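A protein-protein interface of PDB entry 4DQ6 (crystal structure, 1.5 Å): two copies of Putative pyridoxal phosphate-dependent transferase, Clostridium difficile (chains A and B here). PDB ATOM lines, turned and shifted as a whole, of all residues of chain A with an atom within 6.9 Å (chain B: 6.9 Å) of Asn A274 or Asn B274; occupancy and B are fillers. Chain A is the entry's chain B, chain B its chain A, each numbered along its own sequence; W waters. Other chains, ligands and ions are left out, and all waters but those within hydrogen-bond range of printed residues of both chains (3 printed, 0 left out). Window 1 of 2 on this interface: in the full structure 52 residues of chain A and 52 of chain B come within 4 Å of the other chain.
O of Gly B64 sits close to N of Gly A244 (3.3 Å).
The backbone NH (N) of Gly B244 lies close to the backbone carbonyl oxygen (O) of Gly A64.
O of Gly B244 is in hydrogen-bond range of N of Cys A275, 2.8 Å away.
The backbone carbonyl oxygen (O) of Arg A272 lies within hydrogen-bond range of the side-chain amide nitrogen (NE2) of Gln B246, at 3.0 Å.
NE2 of Gln A246 is in hydrogen-bond range of O of Arg B272 (2.9 Å).
The side-chain amide nitrogen (ND2) of Asn B274 sits close to the side-chain amide nitrogen (ND2) of Asn A274 (3.5 Å).
The backbone NH (N) of Cys B275 lies within hydrogen-bond range of the backbone carbonyl oxygen (O) of Gly A244.
O of Thr B66 lies within hydrogen-bond range of NH1 of Arg B272.
The side-chain amide oxygen (OD1) of Asn B274 lies within hydrogen-bond range of the backbone NH (N) of Phe B276 (2.9 Å).
The backbone carbonyl oxygen (O) of Thr A66 sits at hydrogen-bond distance from the guanidinium group (NH1) of Arg A272, at 2.9 Å.
OD1 of Asn A273 sits at hydrogen-bond distance from NH2 of Arg A68.
The side-chain amide nitrogen (ND2) of Asn A274 is in hydrogen-bond range of the backbone carbonyl oxygen (O) of Leu A245, 2.8 Å away.
OD1 of Asn A274 lies within hydrogen-bond range of N of Ser A277 (2.8 Å).
Among the printed residues, merely in contact across the chains: Gly A244 with Asn B274 (3.0 Å), Asn A274 with Gly B244 (3.1 Å), Phe A276 with Phe B276 (3.5 Å), Gln A246 with Asn B274 (3.6 Å), Leu A245 with Phe B276 (3.7 Å), Cys A275 with Leu B245 (3.7 Å), Phe A276 with Leu B245 (3.7 Å), Asn A274 with Gln B246 (3.7 Å), Leu A245 with Cys B275 (3.7 Å), Asn A273 with Gln B246 (3.7 Å) and Gln A246 with Asn B273 (3.7 Å).
Of the printed residues of chain B, Gly A64 touches Gly B244.
Ser A247 touches none of the printed residues of chain B.
Of the printed residues of chain B, Arg A272 touches Gln B246 (3.0 Å).
Printed residues of chain B within 4 Å of Asn A274: Gly B244 (3.1 Å), Gln B246 (3.7 Å) and Asn B274 (3.5 Å).
Of the printed residues of chain A, Arg B272 touches Gln A246 (2.9 Å).
Asn B274 touches just these residues of chain A: Gly A244, Gln A246 and Asn A274.
Printed residues of chain A within 4 Å of Cys B275: Gly A244 (2.9 Å) and Leu A245 (3.7 Å).
Ser B277 touches none of the printed residues of chain A.
The nearest residue of chain B that does not touch Asn A274 is Leu B245 (4.2 Å).
The nearest printed residue of chain A that does not touch Leu B245 is Asn A274 (4.2 Å).
Of the 17 printed residues of chain B, 9 touch a printed residue of chain A.
Hydrophobic or aromatic side chains of chain B within 4 Å of the printed part of chain A: Leu B245 and Phe B276.
Of the 17 printed residues of chain A, 9 touch a printed residue of chain B.
Printed residues of chain A that touch a printed residue of chain B: Gly A64, Gly A244, Leu A245, Gln A246, Arg A272, Asn A273, Asn A274, Cys A275 and Phe A276.
Hydrophobic or aromatic side chains of chain A within 4 Å of the printed part of chain B: Leu A245 and Phe A276.
Among the printed residues, no Asp or Glu carboxylate lies within 4 Å of a Lys or Arg side-chain nitrogen of the other chain.
Gly A244 touches Cys B275, and with the chains exchanged Cys A275 touches Gly B244.
Leu A245 touches Phe B276, and with the chains exchanged Phe A276 touches Leu B245.
Gln A246 touches Asn B274, and with the chains exchanged Asn A274 touches Gln B246.
Phe B276 touches its own counterpart, Phe A276.
Of the 18 pairs that touch across the chains among the printed residues, 18 have their exchanged pair printed and touching as well.
Water W1 lies within hydrogen-bond range of the side-chain hydroxyl of Tyr A95, the side-chain amide oxygen of Gln B246 and the backbone carbonyl oxygen of Arg A272.
Water W2 lies within hydrogen-bond range of the side-chain hydroxyl (OH) of Tyr B95 (2.7 Å), the side-chain amide oxygen (OE1) of Gln A246 (2.9 Å) and the backbone carbonyl oxygen (O) of Arg B272 (3.5 Å).
Water W3 lies within hydrogen-bond range of the side-chain amide oxygen (OE1) of Gln A246 (2.8 Å), the side-chain amide oxygen (OE1) of Gln B246 (2.8 Å), the side-chain amide nitrogen (ND2) of Asn A274 (3.0 Å) and the side-chain amide nitrogen (ND2) of Asn B274 (3.0 Å).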
ATOM      1  N   GLY A  64     -27.992   8.618   9.759  1.00  0.00           N
ATOM      2  CA  GLY A  64     -29.249   9.379   9.760  1.00  0.00           C
ATOM      3  C   GLY A  64     -29.941   9.356  11.085  1.00  0.00           C
ATOM      4  O   GLY A  64     -29.380   9.079  12.134  1.00  0.00           O
ATOM      5  N   THR A  66     -31.698   8.560  14.364  1.00  0.00           N
ATOM      6  CA  THR A  66     -31.545   7.384  15.160  1.00  0.00           C
ATOM      7  C   THR A  66     -32.719   7.061  16.055  1.00  0.00           C
ATOM      8  O   THR A  66     -33.190   7.949  16.820  1.00  0.00           O
ATOM      9  CB  THR A  66     -30.237   7.503  15.975  1.00  0.00           C
ATOM     10  OG1 THR A  66     -29.162   7.786  15.051  1.00  0.00           O
ATOM     11  CG2 THR A  66     -29.879   6.205  16.804  1.00  0.00           C
ATOM     12  N   ARG A  68     -34.394   4.696  19.146  1.00  0.00           N
ATOM     13  CA  ARG A  68     -33.962   4.157  20.436  1.00  0.00           C
ATOM     14  C   ARG A  68     -34.637   2.806  20.633  1.00  0.00           C
ATOM     15  O   ARG A  68     -35.808   2.740  21.020  1.00  0.00           O
ATOM     16  CB  ARG A  68     -34.342   5.162  21.567  1.00  0.00           C
ATOM     17  CG  ARG A  68     -33.762   4.778  22.924  1.00  0.00           C
ATOM     18  CD  ARG A  68     -34.059   5.762  24.060  1.00  0.00           C
ATOM     19  NE  ARG A  68     -33.431   7.020  23.731  1.00  0.00           N
ATOM     20  CZ  ARG A  68     -34.102   8.092  23.238  1.00  0.00           C
ATOM     21  NH1 ARG A  68     -35.410   8.084  23.153  1.00  0.00           N
ATOM     22  NH2 ARG A  68     -33.457   9.129  22.833  1.00  0.00           N
ATOM     23  N   TYR A  95     -34.502  10.390  27.991  1.00  0.00           N
ATOM     24  CA  TYR A  95     -33.192  10.777  27.433  1.00  0.00           C
ATOM     25  C   TYR A  95     -32.927  12.244  27.618  1.00  0.00           C
ATOM     26  O   TYR A  95     -33.782  13.079  27.365  1.00  0.00           O
ATOM     27  CB  TYR A  95     -33.129  10.464  25.911  1.00  0.00           C
ATOM     28  CG  TYR A  95     -32.025  11.130  25.183  1.00  0.00           C
ATOM     29  CD1 TYR A  95     -30.716  10.644  25.254  1.00  0.00           C
ATOM     30  CD2 TYR A  95     -32.230  12.301  24.456  1.00  0.00           C
ATOM     31  CE1 TYR A  95     -29.682  11.332  24.648  1.00  0.00           C
ATOM     32  CE2 TYR A  95     -31.201  12.978  23.872  1.00  0.00           C
ATOM     33  CZ  TYR A  95     -29.933  12.479  23.940  1.00  0.00           C
ATOM     34  OH  TYR A  95     -28.941  13.141  23.320  1.00  0.00           O
ATOM     35  N   ALA A 243     -18.076  11.350  27.881  1.00  0.00           N
ATOM     36  CA  ALA A 243     -18.857  12.626  27.919  1.00  0.00           C
ATOM     37  C   ALA A 243     -18.923  13.222  26.521  1.00  0.00           C
ATOM     38  O   ALA A 243     -19.879  13.941  26.207  1.00  0.00           O
ATOM     39  CB  ALA A 243     -18.178  13.605  28.844  1.00  0.00           C
ATOM     40  N   GLY A 244     -17.923  13.011  25.679  1.00  0.00           N
ATOM     41  CA  GLY A 244     -17.952  13.498  24.309  1.00  0.00           C
ATOM     42  C   GLY A 244     -19.047  12.907  23.446  1.00  0.00           C
ATOM     43  O   GLY A 244     -19.243  13.381  22.315  1.00  0.00           O
ATOM     44  N   LEU A 245     -19.604  11.767  23.880  1.00  0.00           N
ATOM     45  CA  LEU A 245     -20.677  11.088  23.121  1.00  0.00           C
ATOM     46  C   LEU A 245     -22.031  11.643  23.505  1.00  0.00           C
ATOM     47  O   LEU A 245     -22.955  11.595  22.699  1.00  0.00           O
ATOM     48  CB  LEU A 245     -20.660   9.570  23.321  1.00  0.00           C
ATOM     49  CG  LEU A 245     -19.347   8.902  22.894  1.00  0.00           C
ATOM     50  CD1 LEU A 245     -19.349   7.358  23.062  1.00  0.00           C
ATOM     51  CD2 LEU A 245     -18.826   9.295  21.495  1.00  0.00           C
ATOM     52  N   GLN A 246     -22.166  12.212  24.692  1.00  0.00           N
ATOM     53  CA  GLN A 246     -23.362  12.932  25.135  1.00  0.00           C
ATOM     54  C   GLN A 246     -24.543  11.973  25.321  1.00  0.00           C
ATOM     55  O   GLN A 246     -25.226  11.527  24.356  1.00  0.00           O
ATOM     56  CB  GLN A 246     -23.749  14.100  24.202  1.00  0.00           C
ATOM     57  CG  GLN A 246     -22.572  15.024  23.964  1.00  0.00           C
ATOM     58  CD  GLN A 246     -22.924  16.274  23.208  1.00  0.00           C
ATOM     59  OE1 GLN A 246     -23.813  16.293  22.357  1.00  0.00           O
ATOM     60  NE2 GLN A 246     -22.156  17.292  23.425  1.00  0.00           N
ATOM     61  N   SER A 247     -24.699  11.499  26.535  1.00  0.00           N
ATOM     62  CA  SER A 247     -25.775  10.561  26.846  1.00  0.00           C
ATOM     63  C   SER A 247     -26.034  10.629  28.309  1.00  0.00           C
ATOM     64  O   SER A 247     -25.126  10.514  29.100  1.00  0.00           O
ATOM     65  CB  SER A 247     -25.312   9.131  26.501  1.00  0.00           C
ATOM     66  OG  SER A 247     -26.265   8.153  26.905  1.00  0.00           O
ATOM     67  N   ARG A 272     -33.730  12.655  20.372  1.00  0.00           N
ATOM     68  CA  ARG A 272     -32.954  11.487  19.917  1.00  0.00           C
ATOM     69  C   ARG A 272     -31.511  11.492  20.414  1.00  0.00           C
ATOM     70  O   ARG A 272     -30.862  12.520  20.508  1.00  0.00           O
ATOM     71  CB  ARG A 272     -32.927  11.457  18.410  1.00  0.00           C
ATOM     72  CG  ARG A 272     -34.285  11.364  17.751  1.00  0.00           C
ATOM     73  CD  ARG A 272     -34.204  11.029  16.248  1.00  0.00           C
ATOM     74  NE  ARG A 272     -35.570  10.996  15.686  1.00  0.00           N
ATOM     75  CZ  ARG A 272     -36.395   9.947  15.824  1.00  0.00           C
ATOM     76  NH1 ARG A 272     -35.942   8.794  16.320  1.00  0.00           N
ATOM     77  NH2 ARG A 272     -37.606   9.973  15.324  1.00  0.00           N
ATOM     78  N   ASN A 273     -31.016  10.299  20.710  1.00  0.00           N
ATOM     79  CA  ASN A 273     -29.599  10.100  20.904  1.00  0.00           C
ATOM     80  C   ASN A 273     -28.930  10.297  19.522  1.00  0.00           C
ATOM     81  O   ASN A 273     -29.549  10.043  18.487  1.00  0.00           O
ATOM     82  CB  ASN A 273     -29.243   8.642  21.277  1.00  0.00           C
ATOM     83  CG  ASN A 273     -29.596   8.253  22.687  1.00  0.00           C
ATOM     84  OD1 ASN A 273     -30.768   7.988  22.943  1.00  0.00           O
ATOM     85  ND2 ASN A 273     -28.603   8.022  23.519  1.00  0.00           N
ATOM     86  N   ASN A 274     -27.687  10.761  19.532  1.00  0.00           N
ATOM     87  CA  ASN A 274     -26.874  10.670  18.310  1.00  0.00           C
ATOM     88  C   ASN A 274     -26.547   9.186  18.121  1.00  0.00           C
ATOM     89  O   ASN A 274     -26.616   8.329  19.003  1.00  0.00           O
ATOM     90  CB  ASN A 274     -25.640  11.570  18.316  1.00  0.00           C
ATOM     91  CG  ASN A 274     -24.576  11.108  19.269  1.00  0.00           C
ATOM     92  OD1 ASN A 274     -23.987  10.031  19.044  1.00  0.00           O
ATOM     93  ND2 ASN A 274     -24.286  11.887  20.299  1.00  0.00           N
ATOM     94  N   CYS A 275     -26.164   8.903  16.928  1.00  0.00           N
ATOM     95  CA  CYS A 275     -26.047   7.465  16.580  1.00  0.00           C
ATOM     96  C   CYS A 275     -24.958   6.708  17.369  1.00  0.00           C
ATOM     97  O   CYS A 275     -25.013   5.472  17.562  1.00  0.00           O
ATOM     98  CB  CYS A 275     -25.929   7.268  15.065  1.00  0.00           C
ATOM     99  SG  CYS A 275     -24.475   7.998  14.363  1.00  0.00           S
ATOM    100  N   PHE A 276     -23.913   7.419  17.779  1.00  0.00           N
ATOM    101  CA  PHE A 276     -22.821   6.790  18.526  1.00  0.00           C
ATOM    102  C   PHE A 276     -23.103   6.642  20.011  1.00  0.00           C
ATOM    103  O   PHE A 276     -22.794   5.673  20.645  1.00  0.00           O
ATOM    104  CB  PHE A 276     -21.507   7.509  18.216  1.00  0.00           C
ATOM    105  CG  PHE A 276     -21.024   7.269  16.802  1.00  0.00           C
ATOM    106  CD1 PHE A 276     -20.614   5.984  16.380  1.00  0.00           C
ATOM    107  CD2 PHE A 276     -20.949   8.304  15.871  1.00  0.00           C
ATOM    108  CE1 PHE A 276     -20.234   5.811  15.110  1.00  0.00           C
ATOM    109  CE2 PHE A 276     -20.538   8.101  14.593  1.00  0.00           C
ATOM    110  CZ  PHE A 276     -20.133   6.823  14.214  1.00  0.00           C
ATOM    111  N   SER A 277     -23.662   7.680  20.598  1.00  0.00           N
ATOM    112  CA  SER A 277     -24.167   7.635  21.945  1.00  0.00           C
ATOM    113  C   SER A 277     -25.087   6.420  22.177  1.00  0.00           C
ATOM    114  O   SER A 277     -24.999   5.698  23.209  1.00  0.00           O
ATOM    115  CB  SER A 277     -24.953   8.955  22.184  1.00  0.00           C
ATOM    116  OG  SER A 277     -25.819   8.861  23.246  1.00  0.00           O
ATOM    117  N   LEU A 278     -25.986   6.188  21.214  1.00  0.00           N
ATOM    118  CA  LEU A 278     -26.897   5.071  21.337  1.00  0.00           C
ATOM    119  C   LEU A 278     -26.200   3.723  21.571  1.00  0.00           C
ATOM    120  O   LEU A 278     -26.528   3.034  22.535  1.00  0.00           O
ATOM    121  CB  LEU A 278     -27.856   4.971  20.132  1.00  0.00           C
ATOM    122  CG  LEU A 278     -29.018   4.000  20.341  1.00  0.00           C
ATOM    123  CD1 LEU A 278     -30.183   4.840  20.926  1.00  0.00           C
ATOM    124  CD2 LEU A 278     -29.348   3.271  19.015  1.00  0.00           C
ATOM    125  N   VAL A 279     -25.239   3.409  20.713  1.00  0.00           N
ATOM    126  CA  VAL A 279     -24.616   2.117  20.805  1.00  0.00           C
ATOM    127  C   VAL A 279     -23.626   2.043  21.935  1.00  0.00           C
ATOM    128  O   VAL A 279     -23.511   0.996  22.579  1.00  0.00           O
ATOM    129  CB  VAL A 279     -23.976   1.685  19.460  1.00  0.00           C
ATOM    130  CG1 VAL A 279     -25.006   1.613  18.334  1.00  0.00           C
ATOM    131  CG2 VAL A 279     -22.719   2.479  19.088  1.00  0.00           C
ATOM    132  N   GLY B  64     -13.848  12.159  25.485  1.00  0.00           N
ATOM    133  CA  GLY B  64     -14.217  13.113  26.533  1.00  0.00           C
ATOM    134  C   GLY B  64     -14.732  14.416  26.010  1.00  0.00           C
ATOM    135  O   GLY B  64     -15.133  14.554  24.868  1.00  0.00           O
ATOM    136  N   THR B  66     -15.343  17.803  24.379  1.00  0.00           N
ATOM    137  CA  THR B  66     -14.813  18.191  23.101  1.00  0.00           C
ATOM    138  C   THR B  66     -14.722  19.663  22.931  1.00  0.00           C
ATOM    139  O   THR B  66     -15.711  20.338  23.149  1.00  0.00           O
ATOM    140  CB  THR B  66     -15.692  17.600  21.990  1.00  0.00           C
ATOM    141  OG1 THR B  66     -15.717  16.174  22.184  1.00  0.00           O
ATOM    142  CG2 THR B  66     -15.243  17.980  20.572  1.00  0.00           C
ATOM    143  N   ARG B  68     -14.087  23.089  20.477  1.00  0.00           N
ATOM    144  CA  ARG B  68     -14.385  23.485  19.111  1.00  0.00           C
ATOM    145  C   ARG B  68     -13.214  24.308  18.596  1.00  0.00           C
ATOM    146  O   ARG B  68     -13.062  25.497  18.955  1.00  0.00           O
ATOM    147  CB  ARG B  68     -15.695  24.287  19.054  1.00  0.00           C
ATOM    148  CG  ARG B  68     -16.205  24.602  17.649  1.00  0.00           C
ATOM    149  CD  ARG B  68     -17.554  25.323  17.681  1.00  0.00           C
ATOM    150  NE  ARG B  68     -18.555  24.466  18.276  1.00  0.00           N
ATOM    151  CZ  ARG B  68     -19.054  24.600  19.501  1.00  0.00           C
ATOM    152  NH1 ARG B  68     -18.750  25.663  20.250  1.00  0.00           N
ATOM    153  NH2 ARG B  68     -19.832  23.682  19.945  1.00  0.00           N
ATOM    154  N   TYR B  95     -23.296  27.247  17.847  1.00  0.00           N
ATOM    155  CA  TYR B  95     -23.593  25.811  17.705  1.00  0.00           C
ATOM    156  C   TYR B  95     -24.988  25.505  18.243  1.00  0.00           C
ATOM    157  O   TYR B  95     -25.340  25.970  19.337  1.00  0.00           O
ATOM    158  CB  TYR B  95     -22.593  25.011  18.538  1.00  0.00           C
ATOM    159  CG  TYR B  95     -23.021  23.587  18.798  1.00  0.00           C
ATOM    160  CD1 TYR B  95     -22.904  22.587  17.790  1.00  0.00           C
ATOM    161  CD2 TYR B  95     -23.573  23.204  20.008  1.00  0.00           C
ATOM    162  CE1 TYR B  95     -23.371  21.306  17.996  1.00  0.00           C
ATOM    163  CE2 TYR B  95     -24.054  21.913  20.205  1.00  0.00           C
ATOM    164  CZ  TYR B  95     -23.945  20.970  19.216  1.00  0.00           C
ATOM    165  OH  TYR B  95     -24.406  19.665  19.448  1.00  0.00           O
ATOM    166  N   ALA B 243     -27.641  13.587   9.979  1.00  0.00           N
ATOM    167  CA  ALA B 243     -28.616  14.050  11.038  1.00  0.00           C
ATOM    168  C   ALA B 243     -28.355  13.286  12.338  1.00  0.00           C
ATOM    169  O   ALA B 243     -28.554  13.818  13.425  1.00  0.00           O
ATOM    170  CB  ALA B 243     -30.064  13.897  10.610  1.00  0.00           C
ATOM    171  N   GLY B 244     -27.919  12.032  12.217  1.00  0.00           N
ATOM    172  CA  GLY B 244     -27.578  11.192  13.352  1.00  0.00           C
ATOM    173  C   GLY B 244     -26.391  11.672  14.153  1.00  0.00           C
ATOM    174  O   GLY B 244     -26.199  11.210  15.295  1.00  0.00           O
ATOM    175  N   LEU B 245     -25.555  12.544  13.559  1.00  0.00           N
ATOM    176  CA  LEU B 245     -24.414  13.094  14.290  1.00  0.00           C
ATOM    177  C   LEU B 245     -24.770  14.353  15.060  1.00  0.00           C
ATOM    178  O   LEU B 245     -24.077  14.667  16.005  1.00  0.00           O
ATOM    179  CB  LEU B 245     -23.199  13.334  13.381  1.00  0.00           C
ATOM    180  CG  LEU B 245     -22.774  12.140  12.534  1.00  0.00           C
ATOM    181  CD1 LEU B 245     -21.512  12.414  11.715  1.00  0.00           C
ATOM    182  CD2 LEU B 245     -22.533  10.964  13.449  1.00  0.00           C
ATOM    183  N   GLN B 246     -25.866  15.035  14.692  1.00  0.00           N
ATOM    184  CA  GLN B 246     -26.399  16.251  15.372  1.00  0.00           C
ATOM    185  C   GLN B 246     -25.434  17.430  15.348  1.00  0.00           C
ATOM    186  O   GLN B 246     -24.381  17.466  16.059  1.00  0.00           O
ATOM    187  CB  GLN B 246     -26.832  15.918  16.795  1.00  0.00           C
ATOM    188  CG  GLN B 246     -27.716  14.706  16.833  1.00  0.00           C
ATOM    189  CD  GLN B 246     -28.247  14.336  18.206  1.00  0.00           C
ATOM    190  OE1 GLN B 246     -27.596  14.560  19.236  1.00  0.00           O
ATOM    191  NE2 GLN B 246     -29.413  13.727  18.216  1.00  0.00           N
ATOM    192  N   SER B 247     -25.588  18.229  14.345  1.00  0.00           N
ATOM    193  CA  SER B 247     -24.778  19.434  14.216  1.00  0.00           C
ATOM    194  C   SER B 247     -25.549  20.435  13.441  1.00  0.00           C
ATOM    195  O   SER B 247     -26.044  20.134  12.359  1.00  0.00           O
ATOM    196  CB  SER B 247     -23.530  19.076  13.400  1.00  0.00           C
ATOM    197  OG  SER B 247     -22.719  20.210  13.031  1.00  0.00           O
ATOM    198  N   ARG B 272     -21.478  22.169  23.677  1.00  0.00           N
ATOM    199  CA  ARG B 272     -20.409  21.447  22.945  1.00  0.00           C
ATOM    200  C   ARG B 272     -20.948  20.530  21.864  1.00  0.00           C
ATOM    201  O   ARG B 272     -21.971  19.858  22.051  1.00  0.00           O
ATOM    202  CB  ARG B 272     -19.560  20.607  23.929  1.00  0.00           C
ATOM    203  CG  ARG B 272     -18.885  21.350  25.045  1.00  0.00           C
ATOM    204  CD  ARG B 272     -17.892  20.520  25.840  1.00  0.00           C
ATOM    205  NE  ARG B 272     -17.226  21.348  26.816  1.00  0.00           N
ATOM    206  CZ  ARG B 272     -16.217  22.180  26.564  1.00  0.00           C
ATOM    207  NH1 ARG B 272     -15.698  22.306  25.352  1.00  0.00           N
ATOM    208  NH2 ARG B 272     -15.748  22.918  27.545  1.00  0.00           N
ATOM    209  N   ASN B 273     -20.195  20.399  20.750  1.00  0.00           N
ATOM    210  CA  ASN B 273     -20.406  19.332  19.780  1.00  0.00           C
ATOM    211  C   ASN B 273     -20.039  18.023  20.467  1.00  0.00           C
ATOM    212  O   ASN B 273     -19.162  18.002  21.333  1.00  0.00           O
ATOM    213  CB  ASN B 273     -19.454  19.467  18.586  1.00  0.00           C
ATOM    214  CG  ASN B 273     -19.815  20.595  17.636  1.00  0.00           C
ATOM    215  OD1 ASN B 273     -19.628  21.771  17.953  1.00  0.00           O
ATOM    216  ND2 ASN B 273     -20.320  20.239  16.464  1.00  0.00           N
ATOM    217  N   ASN B 274     -20.714  16.939  20.093  1.00  0.00           N
ATOM    218  CA  ASN B 274     -20.159  15.603  20.406  1.00  0.00           C
ATOM    219  C   ASN B 274     -18.935  15.412  19.528  1.00  0.00           C
ATOM    220  O   ASN B 274     -18.697  16.094  18.561  1.00  0.00           O
ATOM    221  CB  ASN B 274     -21.198  14.475  20.281  1.00  0.00           C
ATOM    222  CG  ASN B 274     -21.579  14.178  18.836  1.00  0.00           C
ATOM    223  OD1 ASN B 274     -20.720  13.677  18.098  1.00  0.00           O
ATOM    224  ND2 ASN B 274     -22.834  14.430  18.433  1.00  0.00           N
ATOM    225  N   CYS B 275     -18.108  14.498  19.945  1.00  0.00           N
ATOM    226  CA  CYS B 275     -16.792  14.429  19.322  1.00  0.00           C
ATOM    227  C   CYS B 275     -16.866  14.072  17.856  1.00  0.00           C
ATOM    228  O   CYS B 275     -15.924  14.389  17.103  1.00  0.00           O
ATOM    229  CB  CYS B 275     -15.893  13.482  20.068  1.00  0.00           C
ATOM    230  SG  CYS B 275     -16.445  11.811  20.263  1.00  0.00           S
ATOM    231  N   PHE B 276     -17.908  13.360  17.466  1.00  0.00           N
ATOM    232  CA  PHE B 276     -18.018  12.902  16.079  1.00  0.00           C
ATOM    233  C   PHE B 276     -18.616  13.972  15.168  1.00  0.00           C
ATOM    234  O   PHE B 276     -18.199  14.157  14.035  1.00  0.00           O
ATOM    235  CB  PHE B 276     -18.724  11.566  16.008  1.00  0.00           C
ATOM    236  CG  PHE B 276     -17.912  10.434  16.565  1.00  0.00           C
ATOM    237  CD1 PHE B 276     -16.712  10.082  15.937  1.00  0.00           C
ATOM    238  CD2 PHE B 276     -18.284   9.667  17.682  1.00  0.00           C
ATOM    239  CE1 PHE B 276     -15.931   9.027  16.383  1.00  0.00           C
ATOM    240  CE2 PHE B 276     -17.464   8.614  18.172  1.00  0.00           C
ATOM    241  CZ  PHE B 276     -16.279   8.284  17.471  1.00  0.00           C
ATOM    242  N   SER B 277     -19.649  14.647  15.629  1.00  0.00           N
ATOM    243  CA  SER B 277     -20.169  15.777  14.938  1.00  0.00           C
ATOM    244  C   SER B 277     -19.096  16.823  14.599  1.00  0.00           C
ATOM    245  O   SER B 277     -19.072  17.413  13.508  1.00  0.00           O
ATOM    246  CB  SER B 277     -21.270  16.393  15.856  1.00  0.00           C
ATOM    247  OG  SER B 277     -21.559  17.698  15.635  1.00  0.00           O
ATOM    248  N   LEU B 278     -18.202  17.064  15.556  1.00  0.00           N
ATOM    249  CA  LEU B 278     -17.159  18.062  15.360  1.00  0.00           C
ATOM    250  C   LEU B 278     -16.333  17.768  14.123  1.00  0.00           C
ATOM    251  O   LEU B 278     -16.146  18.631  13.243  1.00  0.00           O
ATOM    252  CB  LEU B 278     -16.187  18.090  16.526  1.00  0.00           C
ATOM    253  CG  LEU B 278     -15.230  19.264  16.476  1.00  0.00           C
ATOM    254  CD1 LEU B 278     -15.934  20.473  17.132  1.00  0.00           C
ATOM    255  CD2 LEU B 278     -13.933  18.956  17.225  1.00  0.00           C
ATOM    256  N   VAL B 279     -15.859  16.543  14.048  1.00  0.00           N
ATOM    257  CA  VAL B 279     -14.953  16.200  12.937  1.00  0.00           C
ATOM    258  C   VAL B 279     -15.680  16.007  11.622  1.00  0.00           C
ATOM    259  O   VAL B 279     -15.152  16.359  10.564  1.00  0.00           O
ATOM    260  CB  VAL B 279     -14.031  14.980  13.241  1.00  0.00           C
ATOM    261  CG1 VAL B 279     -13.155  15.194  14.481  1.00  0.00           C
ATOM    262  CG2 VAL B 279     -14.824  13.691  13.243  1.00  0.00           C
HETATM  263  O   HOH W   1     -29.038  15.203  21.670  1.00  0.00           O
HETATM  264  O   HOH W   2     -25.254  18.770  21.872  1.00  0.00           O
HETATM  265  O   HOH W   3     -25.076  14.780  20.404  1.00  0.00           O
